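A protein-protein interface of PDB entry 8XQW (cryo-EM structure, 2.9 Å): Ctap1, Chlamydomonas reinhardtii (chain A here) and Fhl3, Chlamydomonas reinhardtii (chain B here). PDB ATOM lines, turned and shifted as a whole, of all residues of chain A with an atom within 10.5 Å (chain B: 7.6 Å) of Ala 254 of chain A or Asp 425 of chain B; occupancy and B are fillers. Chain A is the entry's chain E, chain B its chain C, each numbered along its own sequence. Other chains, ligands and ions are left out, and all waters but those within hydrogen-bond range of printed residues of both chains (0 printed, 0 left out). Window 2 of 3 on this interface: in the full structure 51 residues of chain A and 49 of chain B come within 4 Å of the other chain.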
ATOM      1  N   TYR A 182      27.606   2.983  -9.397  1.00  0.00           N
ATOM      2  CA  TYR A 182      26.663   1.996  -9.901  1.00  0.00           C
ATOM      3  C   TYR A 182      25.494   2.667 -10.597  1.00  0.00           C
ATOM      4  O   TYR A 182      25.097   2.263 -11.693  1.00  0.00           O
ATOM      5  CB  TYR A 182      26.163   1.125  -8.762  1.00  0.00           C
ATOM      6  CG  TYR A 182      25.233   0.035  -9.205  1.00  0.00           C
ATOM      7  CD1 TYR A 182      25.692  -1.016  -9.960  1.00  0.00           C
ATOM      8  CD2 TYR A 182      23.899   0.057  -8.863  1.00  0.00           C
ATOM      9  CE1 TYR A 182      24.852  -2.009 -10.362  1.00  0.00           C
ATOM     10  CE2 TYR A 182      23.055  -0.935  -9.262  1.00  0.00           C
ATOM     11  CZ  TYR A 182      23.537  -1.964 -10.011  1.00  0.00           C
ATOM     12  OH  TYR A 182      22.694  -2.963 -10.416  1.00  0.00           O
ATOM     13  N   ARG A 186      24.486   2.478 -14.534  1.00  0.00           N
ATOM     14  CA  ARG A 186      23.184   2.032 -15.010  1.00  0.00           C
ATOM     15  C   ARG A 186      22.576   3.050 -15.958  1.00  0.00           C
ATOM     16  O   ARG A 186      21.933   2.682 -16.946  1.00  0.00           O
ATOM     17  CB  ARG A 186      22.246   1.782 -13.840  1.00  0.00           C
ATOM     18  CG  ARG A 186      22.122   0.340 -13.483  1.00  0.00           C
ATOM     19  CD  ARG A 186      20.899   0.104 -12.650  1.00  0.00           C
ATOM     20  NE  ARG A 186      20.668   1.210 -11.737  1.00  0.00           N
ATOM     21  CZ  ARG A 186      19.729   1.213 -10.802  1.00  0.00           C
ATOM     22  NH1 ARG A 186      18.944   0.159 -10.656  1.00  0.00           N
ATOM     23  NH2 ARG A 186      19.580   2.262 -10.009  1.00  0.00           N
ATOM     24  N   GLY A 242      31.406  -7.268  -3.648  1.00  0.00           N
ATOM     25  CA  GLY A 242      30.271  -7.167  -2.758  1.00  0.00           C
ATOM     26  C   GLY A 242      29.509  -8.456  -2.603  1.00  0.00           C
ATOM     27  O   GLY A 242      29.597  -9.112  -1.567  1.00  0.00           O
ATOM     28  N   GLU A 243      28.777  -8.841  -3.629  1.00  0.00           N
ATOM     29  CA  GLU A 243      28.098 -10.120  -3.653  1.00  0.00           C
ATOM     30  C   GLU A 243      28.215 -10.694  -5.051  1.00  0.00           C
ATOM     31  O   GLU A 243      28.071  -9.982  -6.044  1.00  0.00           O
ATOM     32  CB  GLU A 243      26.640  -9.997  -3.240  1.00  0.00           C
ATOM     33  CG  GLU A 243      25.810  -9.128  -4.132  1.00  0.00           C
ATOM     34  CD  GLU A 243      24.406  -9.651  -4.284  1.00  0.00           C
ATOM     35  OE1 GLU A 243      23.814  -9.473  -5.367  1.00  0.00           O
ATOM     36  OE2 GLU A 243      23.902 -10.263  -3.325  1.00  0.00           O
ATOM     37  N   VAL A 245      27.660 -12.071  -8.457  1.00  0.00           N
ATOM     38  CA  VAL A 245      26.598 -12.135  -9.447  1.00  0.00           C
ATOM     39  C   VAL A 245      27.223 -12.441 -10.795  1.00  0.00           C
ATOM     40  O   VAL A 245      28.400 -12.175 -11.033  1.00  0.00           O
ATOM     41  CB  VAL A 245      25.778 -10.835  -9.540  1.00  0.00           C
ATOM     42  CG1 VAL A 245      25.252 -10.442  -8.197  1.00  0.00           C
ATOM     43  CG2 VAL A 245      26.613  -9.735 -10.116  1.00  0.00           C
ATOM     44  N   GLU A 249      23.246  -9.840 -15.285  1.00  0.00           N
ATOM     45  CA  GLU A 249      22.412  -9.678 -14.103  1.00  0.00           C
ATOM     46  C   GLU A 249      22.029  -8.218 -13.940  1.00  0.00           C
ATOM     47  O   GLU A 249      22.895  -7.341 -13.956  1.00  0.00           O
ATOM     48  CB  GLU A 249      23.138 -10.175 -12.864  1.00  0.00           C
ATOM     49  CG  GLU A 249      22.236 -10.814 -11.853  1.00  0.00           C
ATOM     50  CD  GLU A 249      21.535  -9.800 -10.993  1.00  0.00           C
ATOM     51  OE1 GLU A 249      20.606 -10.177 -10.249  1.00  0.00           O
ATOM     52  OE2 GLU A 249      21.913  -8.617 -11.060  1.00  0.00           O
ATOM     53  N   GLN A 250      20.737  -7.961 -13.759  1.00  0.00           N
ATOM     54  CA  GLN A 250      20.204  -6.618 -13.546  1.00  0.00           C
ATOM     55  C   GLN A 250      19.279  -6.654 -12.341  1.00  0.00           C
ATOM     56  O   GLN A 250      18.070  -6.828 -12.480  1.00  0.00           O
ATOM     57  CB  GLN A 250      19.487  -6.140 -14.750  1.00  0.00           C
ATOM     58  CG  GLN A 250      20.302  -6.182 -16.000  1.00  0.00           C
ATOM     59  CD  GLN A 250      19.445  -6.291 -17.220  1.00  0.00           C
ATOM     60  OE1 GLN A 250      19.733  -5.695 -18.252  1.00  0.00           O
ATOM     61  NE2 GLN A 250      18.377  -7.061 -17.114  1.00  0.00           N
ATOM     62  N   ALA A 251      19.848  -6.491 -11.161  1.00  0.00           N
ATOM     63  CA  ALA A 251      19.064  -6.356  -9.945  1.00  0.00           C
ATOM     64  C   ALA A 251      19.965  -5.853  -8.830  1.00  0.00           C
ATOM     65  O   ALA A 251      21.010  -6.455  -8.566  1.00  0.00           O
ATOM     66  CB  ALA A 251      18.424  -7.685  -9.549  1.00  0.00           C
ATOM     67  N   PRO A 252      19.597  -4.777  -8.147  1.00  0.00           N
ATOM     68  CA  PRO A 252      20.435  -4.262  -7.071  1.00  0.00           C
ATOM     69  C   PRO A 252      20.493  -5.249  -5.922  1.00  0.00           C
ATOM     70  O   PRO A 252      19.626  -6.126  -5.802  1.00  0.00           O
ATOM     71  CB  PRO A 252      19.726  -2.963  -6.662  1.00  0.00           C
ATOM     72  CG  PRO A 252      18.823  -2.642  -7.796  1.00  0.00           C
ATOM     73  CD  PRO A 252      18.402  -3.950  -8.354  1.00  0.00           C
ATOM     74  N   PRO A 253      21.467  -5.111  -4.985  1.00  0.00           N
ATOM     75  CA  PRO A 253      21.655  -6.125  -3.961  1.00  0.00           C
ATOM     76  C   PRO A 253      20.956  -6.037  -2.621  1.00  0.00           C
ATOM     77  O   PRO A 253      21.564  -6.537  -1.666  1.00  0.00           O
ATOM     78  CB  PRO A 253      23.160  -5.906  -3.789  1.00  0.00           C
ATOM     79  CG  PRO A 253      23.288  -4.426  -3.649  1.00  0.00           C
ATOM     80  CD  PRO A 253      22.411  -3.984  -4.791  1.00  0.00           C
ATOM     81  N   ALA A 254      19.773  -5.430  -2.537  1.00  0.00           N
ATOM     82  CA  ALA A 254      18.979  -5.397  -1.278  1.00  0.00           C
ATOM     83  C   ALA A 254      19.574  -4.435  -0.252  1.00  0.00           C
ATOM     84  O   ALA A 254      18.876  -4.121   0.729  1.00  0.00           O
ATOM     85  CB  ALA A 254      18.828  -6.779  -0.688  1.00  0.00           C
ATOM     86  N   SER A 255      20.799  -3.977  -0.466  1.00  0.00           N
ATOM     87  CA  SER A 255      21.397  -2.976   0.444  1.00  0.00           C
ATOM     88  C   SER A 255      22.431  -2.187  -0.346  1.00  0.00           C
ATOM     89  O   SER A 255      23.386  -2.797  -0.826  1.00  0.00           O
ATOM     90  CB  SER A 255      22.045  -3.637   1.608  1.00  0.00           C
ATOM     91  OG  SER A 255      23.279  -3.008   1.918  1.00  0.00           O
ATOM     92  N   PRO A 256      22.310  -0.863  -0.478  1.00  0.00           N
ATOM     93  CA  PRO A 256      23.350  -0.110  -1.155  1.00  0.00           C
ATOM     94  C   PRO A 256      24.773  -0.352  -0.671  1.00  0.00           C
ATOM     95  O   PRO A 256      25.685   0.288  -1.207  1.00  0.00           O
ATOM     96  CB  PRO A 256      22.887   1.311  -0.853  1.00  0.00           C
ATOM     97  CG  PRO A 256      21.388   1.196  -0.806  1.00  0.00           C
ATOM     98  CD  PRO A 256      21.175  -0.087  -0.032  1.00  0.00           C
ATOM     99  N   ALA A 257      24.979  -1.231   0.307  1.00  0.00           N
ATOM    100  CA  ALA A 257      26.325  -1.430   0.884  1.00  0.00           C
ATOM    101  C   ALA A 257      26.953  -2.708   0.337  1.00  0.00           C
ATOM    102  O   ALA A 257      28.113  -2.988   0.668  1.00  0.00           O
ATOM    103  CB  ALA A 257      26.192  -1.477   2.375  1.00  0.00           C
ATOM    104  N   ASP A 258      26.212  -3.455  -0.473  1.00  0.00           N
ATOM    105  CA  ASP A 258      26.709  -4.718  -1.066  1.00  0.00           C
ATOM    106  C   ASP A 258      27.076  -4.488  -2.529  1.00  0.00           C
ATOM    107  O   ASP A 258      26.913  -5.417  -3.323  1.00  0.00           O
ATOM    108  CB  ASP A 258      25.644  -5.790  -1.008  1.00  0.00           C
ATOM    109  CG  ASP A 258      24.753  -5.769   0.223  1.00  0.00           C
ATOM    110  OD1 ASP A 258      25.050  -4.993   1.150  1.00  0.00           O
ATOM    111  OD2 ASP A 258      23.775  -6.539   0.249  1.00  0.00           O
ATOM    112  N   ILE A 259      27.513  -3.283  -2.874  1.00  0.00           N
ATOM    113  CA  ILE A 259      27.964  -3.011  -4.265  1.00  0.00           C
ATOM    114  C   ILE A 259      29.488  -3.092  -4.272  1.00  0.00           C
ATOM    115  O   ILE A 259      30.126  -2.238  -3.656  1.00  0.00           O
ATOM    116  CB  ILE A 259      27.427  -1.679  -4.812  1.00  0.00           C
ATOM    117  CG1 ILE A 259      25.916  -1.626  -4.737  1.00  0.00           C
ATOM    118  CG2 ILE A 259      27.921  -1.439  -6.235  1.00  0.00           C
ATOM    119  CD1 ILE A 259      25.236  -2.136  -5.990  1.00  0.00           C
ATOM    120  N   HIS A 263      29.263  -6.220  -9.317  1.00  0.00           N
ATOM    121  CA  HIS A 263      28.164  -5.494  -9.941  1.00  0.00           C
ATOM    122  C   HIS A 263      28.673  -4.474 -10.947  1.00  0.00           C
ATOM    123  O   HIS A 263      28.085  -4.297 -12.018  1.00  0.00           O
ATOM    124  CB  HIS A 263      27.327  -4.799  -8.880  1.00  0.00           C
ATOM    125  CG  HIS A 263      26.227  -5.641  -8.332  1.00  0.00           C
ATOM    126  ND1 HIS A 263      25.059  -5.873  -9.021  1.00  0.00           N
ATOM    127  CD2 HIS A 263      26.104  -6.291  -7.153  1.00  0.00           C
ATOM    128  CE1 HIS A 263      24.268  -6.639  -8.296  1.00  0.00           C
ATOM    129  NE2 HIS A 263      24.877  -6.903  -7.155  1.00  0.00           N
ATOM    130  N   TYR B 378      10.655   2.853   9.790  1.00  0.00           N
ATOM    131  CA  TYR B 378      11.187   2.586   8.464  1.00  0.00           C
ATOM    132  C   TYR B 378      10.483   3.495   7.466  1.00  0.00           C
ATOM    133  O   TYR B 378      10.873   3.591   6.299  1.00  0.00           O
ATOM    134  CB  TYR B 378      11.011   1.111   8.105  1.00  0.00           C
ATOM    135  CG  TYR B 378      11.639   0.718   6.794  1.00  0.00           C
ATOM    136  CD1 TYR B 378      12.774   1.355   6.329  1.00  0.00           C
ATOM    137  CD2 TYR B 378      11.086  -0.280   6.007  1.00  0.00           C
ATOM    138  CE1 TYR B 378      13.340   1.011   5.125  1.00  0.00           C
ATOM    139  CE2 TYR B 378      11.647  -0.633   4.803  1.00  0.00           C
ATOM    140  CZ  TYR B 378      12.773   0.018   4.368  1.00  0.00           C
ATOM    141  OH  TYR B 378      13.343  -0.328   3.171  1.00  0.00           O
ATOM    142  N   TRP B 382      11.126   6.923   4.666  1.00  0.00           N
ATOM    143  CA  TRP B 382      10.711   6.895   3.270  1.00  0.00           C
ATOM    144  C   TRP B 382      10.111   8.230   2.855  1.00  0.00           C
ATOM    145  O   TRP B 382      10.513   8.818   1.847  1.00  0.00           O
ATOM    146  CB  TRP B 382       9.715   5.758   3.049  1.00  0.00           C
ATOM    147  CG  TRP B 382       9.703   5.253   1.647  1.00  0.00           C
ATOM    148  CD1 TRP B 382       9.096   5.829   0.575  1.00  0.00           C
ATOM    149  CD2 TRP B 382      10.339   4.069   1.159  1.00  0.00           C
ATOM    150  NE1 TRP B 382       9.308   5.076  -0.550  1.00  0.00           N
ATOM    151  CE2 TRP B 382      10.070   3.989  -0.218  1.00  0.00           C
ATOM    152  CE3 TRP B 382      11.110   3.068   1.754  1.00  0.00           C
ATOM    153  CZ2 TRP B 382      10.547   2.950  -1.010  1.00  0.00           C
ATOM    154  CZ3 TRP B 382      11.582   2.038   0.966  1.00  0.00           C
ATOM    155  CH2 TRP B 382      11.299   1.987  -0.400  1.00  0.00           C
ATOM    156  N   PHE B 395      25.748   3.786   6.085  1.00  0.00           N
ATOM    157  CA  PHE B 395      25.341   2.446   6.466  1.00  0.00           C
ATOM    158  C   PHE B 395      26.292   1.875   7.502  1.00  0.00           C
ATOM    159  O   PHE B 395      27.499   2.117   7.466  1.00  0.00           O
ATOM    160  CB  PHE B 395      25.291   1.536   5.244  1.00  0.00           C
ATOM    161  CG  PHE B 395      24.196   1.877   4.300  1.00  0.00           C
ATOM    162  CD1 PHE B 395      24.394   2.791   3.293  1.00  0.00           C
ATOM    163  CD2 PHE B 395      22.954   1.303   4.439  1.00  0.00           C
ATOM    164  CE1 PHE B 395      23.377   3.115   2.438  1.00  0.00           C
ATOM    165  CE2 PHE B 395      21.939   1.625   3.585  1.00  0.00           C
ATOM    166  CZ  PHE B 395      22.150   2.533   2.587  1.00  0.00           C
ATOM    167  N   LYS B 400      25.160  -4.878   8.031  1.00  0.00           N
ATOM    168  CA  LYS B 400      24.889  -3.792   7.090  1.00  0.00           C
ATOM    169  C   LYS B 400      23.394  -3.619   6.851  1.00  0.00           C
ATOM    170  O   LYS B 400      22.919  -3.658   5.717  1.00  0.00           O
ATOM    171  CB  LYS B 400      25.625  -4.012   5.769  1.00  0.00           C
ATOM    172  CG  LYS B 400      27.128  -4.007   5.898  1.00  0.00           C
ATOM    173  CD  LYS B 400      27.644  -2.612   6.183  1.00  0.00           C
ATOM    174  CE  LYS B 400      29.148  -2.616   6.378  1.00  0.00           C
ATOM    175  NZ  LYS B 400      29.710  -1.242   6.430  1.00  0.00           N
ATOM    176  N   ASN B 401      22.642  -3.433   7.932  1.00  0.00           N
ATOM    177  CA  ASN B 401      21.217  -3.157   7.831  1.00  0.00           C
ATOM    178  C   ASN B 401      20.770  -2.055   8.782  1.00  0.00           C
ATOM    179  O   ASN B 401      19.594  -2.015   9.154  1.00  0.00           O
ATOM    180  CB  ASN B 401      20.404  -4.431   8.080  1.00  0.00           C
ATOM    181  CG  ASN B 401      20.401  -4.845   9.532  1.00  0.00           C
ATOM    182  OD1 ASN B 401      21.346  -4.569  10.268  1.00  0.00           O
ATOM    183  ND2 ASN B 401      19.334  -5.504   9.956  1.00  0.00           N
ATOM    184  N   LEU B 422      17.054  -1.268   8.729  1.00  0.00           N
ATOM    185  CA  LEU B 422      16.659  -1.581   7.338  1.00  0.00           C
ATOM    186  C   LEU B 422      16.321  -3.056   7.190  1.00  0.00           C
ATOM    187  O   LEU B 422      17.203  -3.892   7.441  1.00  0.00           O
ATOM    188  CB  LEU B 422      17.852  -1.243   6.460  1.00  0.00           C
ATOM    189  CG  LEU B 422      18.118   0.238   6.205  1.00  0.00           C
ATOM    190  CD1 LEU B 422      18.941   0.248   4.939  1.00  0.00           C
ATOM    191  CD2 LEU B 422      16.821   0.997   6.014  1.00  0.00           C
ATOM    192  N   PRO B 423      15.079  -3.419   6.835  1.00  0.00           N
ATOM    193  CA  PRO B 423      14.772  -4.802   6.519  1.00  0.00           C
ATOM    194  C   PRO B 423      14.814  -4.938   4.994  1.00  0.00           C
ATOM    195  O   PRO B 423      14.093  -4.206   4.289  1.00  0.00           O
ATOM    196  CB  PRO B 423      13.383  -4.941   7.125  1.00  0.00           C
ATOM    197  CG  PRO B 423      12.809  -3.532   7.139  1.00  0.00           C
ATOM    198  CD  PRO B 423      13.929  -2.548   6.849  1.00  0.00           C
ATOM    199  N   PRO B 424      15.638  -5.844   4.422  1.00  0.00           N
ATOM    200  CA  PRO B 424      15.796  -5.962   2.973  1.00  0.00           C
ATOM    201  C   PRO B 424      14.726  -5.398   2.030  1.00  0.00           C
ATOM    202  O   PRO B 424      13.599  -5.924   2.003  1.00  0.00           O
ATOM    203  CB  PRO B 424      15.883  -7.488   2.890  1.00  0.00           C
ATOM    204  CG  PRO B 424      16.760  -7.846   4.066  1.00  0.00           C
ATOM    205  CD  PRO B 424      16.440  -6.816   5.139  1.00  0.00           C
ATOM    206  N   ASP B 425      15.088  -4.377   1.244  1.00  0.00           N
ATOM    207  CA  ASP B 425      14.151  -3.774   0.255  1.00  0.00           C
ATOM    208  C   ASP B 425      14.946  -3.314  -0.972  1.00  0.00           C
ATOM    209  O   ASP B 425      15.607  -2.262  -0.894  1.00  0.00           O
ATOM    210  CB  ASP B 425      13.362  -2.631   0.864  1.00  0.00           C
ATOM    211  CG  ASP B 425      12.270  -2.018  -0.003  1.00  0.00           C
ATOM    212  OD1 ASP B 425      12.293  -2.226  -1.236  1.00  0.00           O
ATOM    213  OD2 ASP B 425      11.399  -1.329   0.564  1.00  0.00           O
ATOM    214  N   PRO B 426      14.879  -4.038  -2.106  1.00  0.00           N
ATOM    215  CA  PRO B 426      15.645  -3.679  -3.294  1.00  0.00           C
ATOM    216  C   PRO B 426      15.262  -2.383  -4.000  1.00  0.00           C
ATOM    217  O   PRO B 426      15.910  -2.044  -5.002  1.00  0.00           O
ATOM    218  CB  PRO B 426      15.389  -4.900  -4.183  1.00  0.00           C
ATOM    219  CG  PRO B 426      14.021  -5.369  -3.769  1.00  0.00           C
ATOM    220  CD  PRO B 426      14.072  -5.233  -2.264  1.00  0.00           C
ATOM    221  N   GLU B 427      14.231  -1.685  -3.526  1.00  0.00           N
ATOM    222  CA  GLU B 427      13.883  -0.394  -4.100  1.00  0.00           C
ATOM    223  C   GLU B 427      14.631   0.750  -3.432  1.00  0.00           C
ATOM    224  O   GLU B 427      14.584   1.883  -3.923  1.00  0.00           O
ATOM    225  CB  GLU B 427      12.369  -0.179  -3.993  1.00  0.00           C
ATOM    226  CG  GLU B 427      11.814   1.053  -4.702  1.00  0.00           C
ATOM    227  CD  GLU B 427      12.348   1.224  -6.107  1.00  0.00           C
ATOM    228  OE1 GLU B 427      13.248   2.067  -6.300  1.00  0.00           O
ATOM    229  OE2 GLU B 427      11.866   0.521  -7.019  1.00  0.00           O
ATOM    230  N   LEU B 428      15.346   0.469  -2.344  1.00  0.00           N
ATOM    231  CA  LEU B 428      15.946   1.531  -1.549  1.00  0.00           C
ATOM    232  C   LEU B 428      16.960   2.337  -2.348  1.00  0.00           C
ATOM    233  O   LEU B 428      16.922   3.572  -2.339  1.00  0.00           O
ATOM    234  CB  LEU B 428      16.598   0.934  -0.308  1.00  0.00           C
ATOM    235  CG  LEU B 428      17.277   1.919   0.635  1.00  0.00           C
ATOM    236  CD1 LEU B 428      16.356   3.070   0.955  1.00  0.00           C
ATOM    237  CD2 LEU B 428      17.692   1.210   1.902  1.00  0.00           C
ATOM    238  N   LEU B 429      17.868   1.662  -3.051  1.00  0.00           N
ATOM    239  CA  LEU B 429      18.998   2.360  -3.654  1.00  0.00           C
ATOM    240  C   LEU B 429      18.540   3.337  -4.724  1.00  0.00           C
ATOM    241  O   LEU B 429      19.040   4.465  -4.804  1.00  0.00           O
ATOM    242  CB  LEU B 429      19.985   1.352  -4.235  1.00  0.00           C
ATOM    243  CG  LEU B 429      21.033   1.899  -5.204  1.00  0.00           C
ATOM    244  CD1 LEU B 429      21.870   2.973  -4.557  1.00  0.00           C
ATOM    245  CD2 LEU B 429      21.911   0.776  -5.692  1.00  0.00           C
ATOM    246  N   ASP B 430      17.601   2.916  -5.564  1.00  0.00           N
ATOM    247  CA  ASP B 430      17.091   3.801  -6.606  1.00  0.00           C
ATOM    248  C   ASP B 430      16.364   4.992  -6.000  1.00  0.00           C
ATOM    249  O   ASP B 430      16.521   6.127  -6.462  1.00  0.00           O
ATOM    250  CB  ASP B 430      16.173   3.011  -7.537  1.00  0.00           C
ATOM    251  CG  ASP B 430      16.126   1.532  -7.189  1.00  0.00           C
ATOM    252  OD1 ASP B 430      16.371   1.187  -6.013  1.00  0.00           O
ATOM    253  OD2 ASP B 430      15.850   0.711  -8.084  1.00  0.00           O
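The side-chain carboxylate (OD2) of Asp 425 of chain B sits close to the side-chain hydroxyl (OH) of Tyr 378 of chain B.
The side-chain carboxylate of Asp 425 of chain B sits at hydrogen-bond distance from the backbone NH of Glu 427 of chain B, 3.0 Å away.
OG of Ser 255 of chain A sits at hydrogen-bond distance from OD1 of Asp 258 of chain A, 2.8 Å away.
The backbone NH of Ala 257 of chain A lies close to the side-chain hydroxyl of Ser 255 of chain A, at 2.9 Å.
Of the 14 printed residues of chain B, 4 touch a printed residue of chain A.
Printed residues of chain A that touch a printed residue of chain B: Tyr 182, Ala 254, Ser 255 and Pro 256.
Among the printed residues, 5 pairs touch across the chains.
Among the printed residues, no Asp or Glu carboxylate lies within 4 Å of a Lys or Arg side-chain nitrogen of the other chain.
Printed residues of chain B within 4 Å of Tyr 182 of chain A: Leu 429.
Printed residues of chain B within 4 Å of Ala 254 of chain A: Asp 425.
Printed residues of chain B within 4 Å of Pro 256 of chain A: Phe 395 (3.7 Å) and Leu 429 (3.7 Å).
Ile 259 of chain A touches none of the printed residues of chain B.
Of the printed residues of chain A, Lys 400 of chain B touches Ser 255 (3.9 Å).
No residue of chain A comes within 4 Å of Pro 423 of chain B.
No residue of chain A comes within 4 Å of Pro 424 of chain B.
Of chain A, only Ala 254 comes within 4 Å of Asp 425 of chain B.
Leu 428 of chain B touches none of the printed residues of chain A.
The nearest printed residue of chain B that does not touch Ala 254 of chain A is Pro 424 of chain B (4.2 Å).
The nearest residue of chain A that does not touch Asp 425 of chain B is Ser 255 of chain A (5.5 Å).
CD2 of Leu 429 of chain B touches CD2 of Tyr 182 of chain A, at 3.8 Å.
O of Ala 254 of chain A touches N of Asp 425 of chain B (3.8 Å).
Ser 255 of chain A touches Lys 400 of chain B.
CZ of Phe 395 of chain B touches CB of Pro 256 of chain A, at 3.7 Å.
CG of Pro 256 of chain A touches CB of Leu 429 of chain B, at 3.7 Å.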
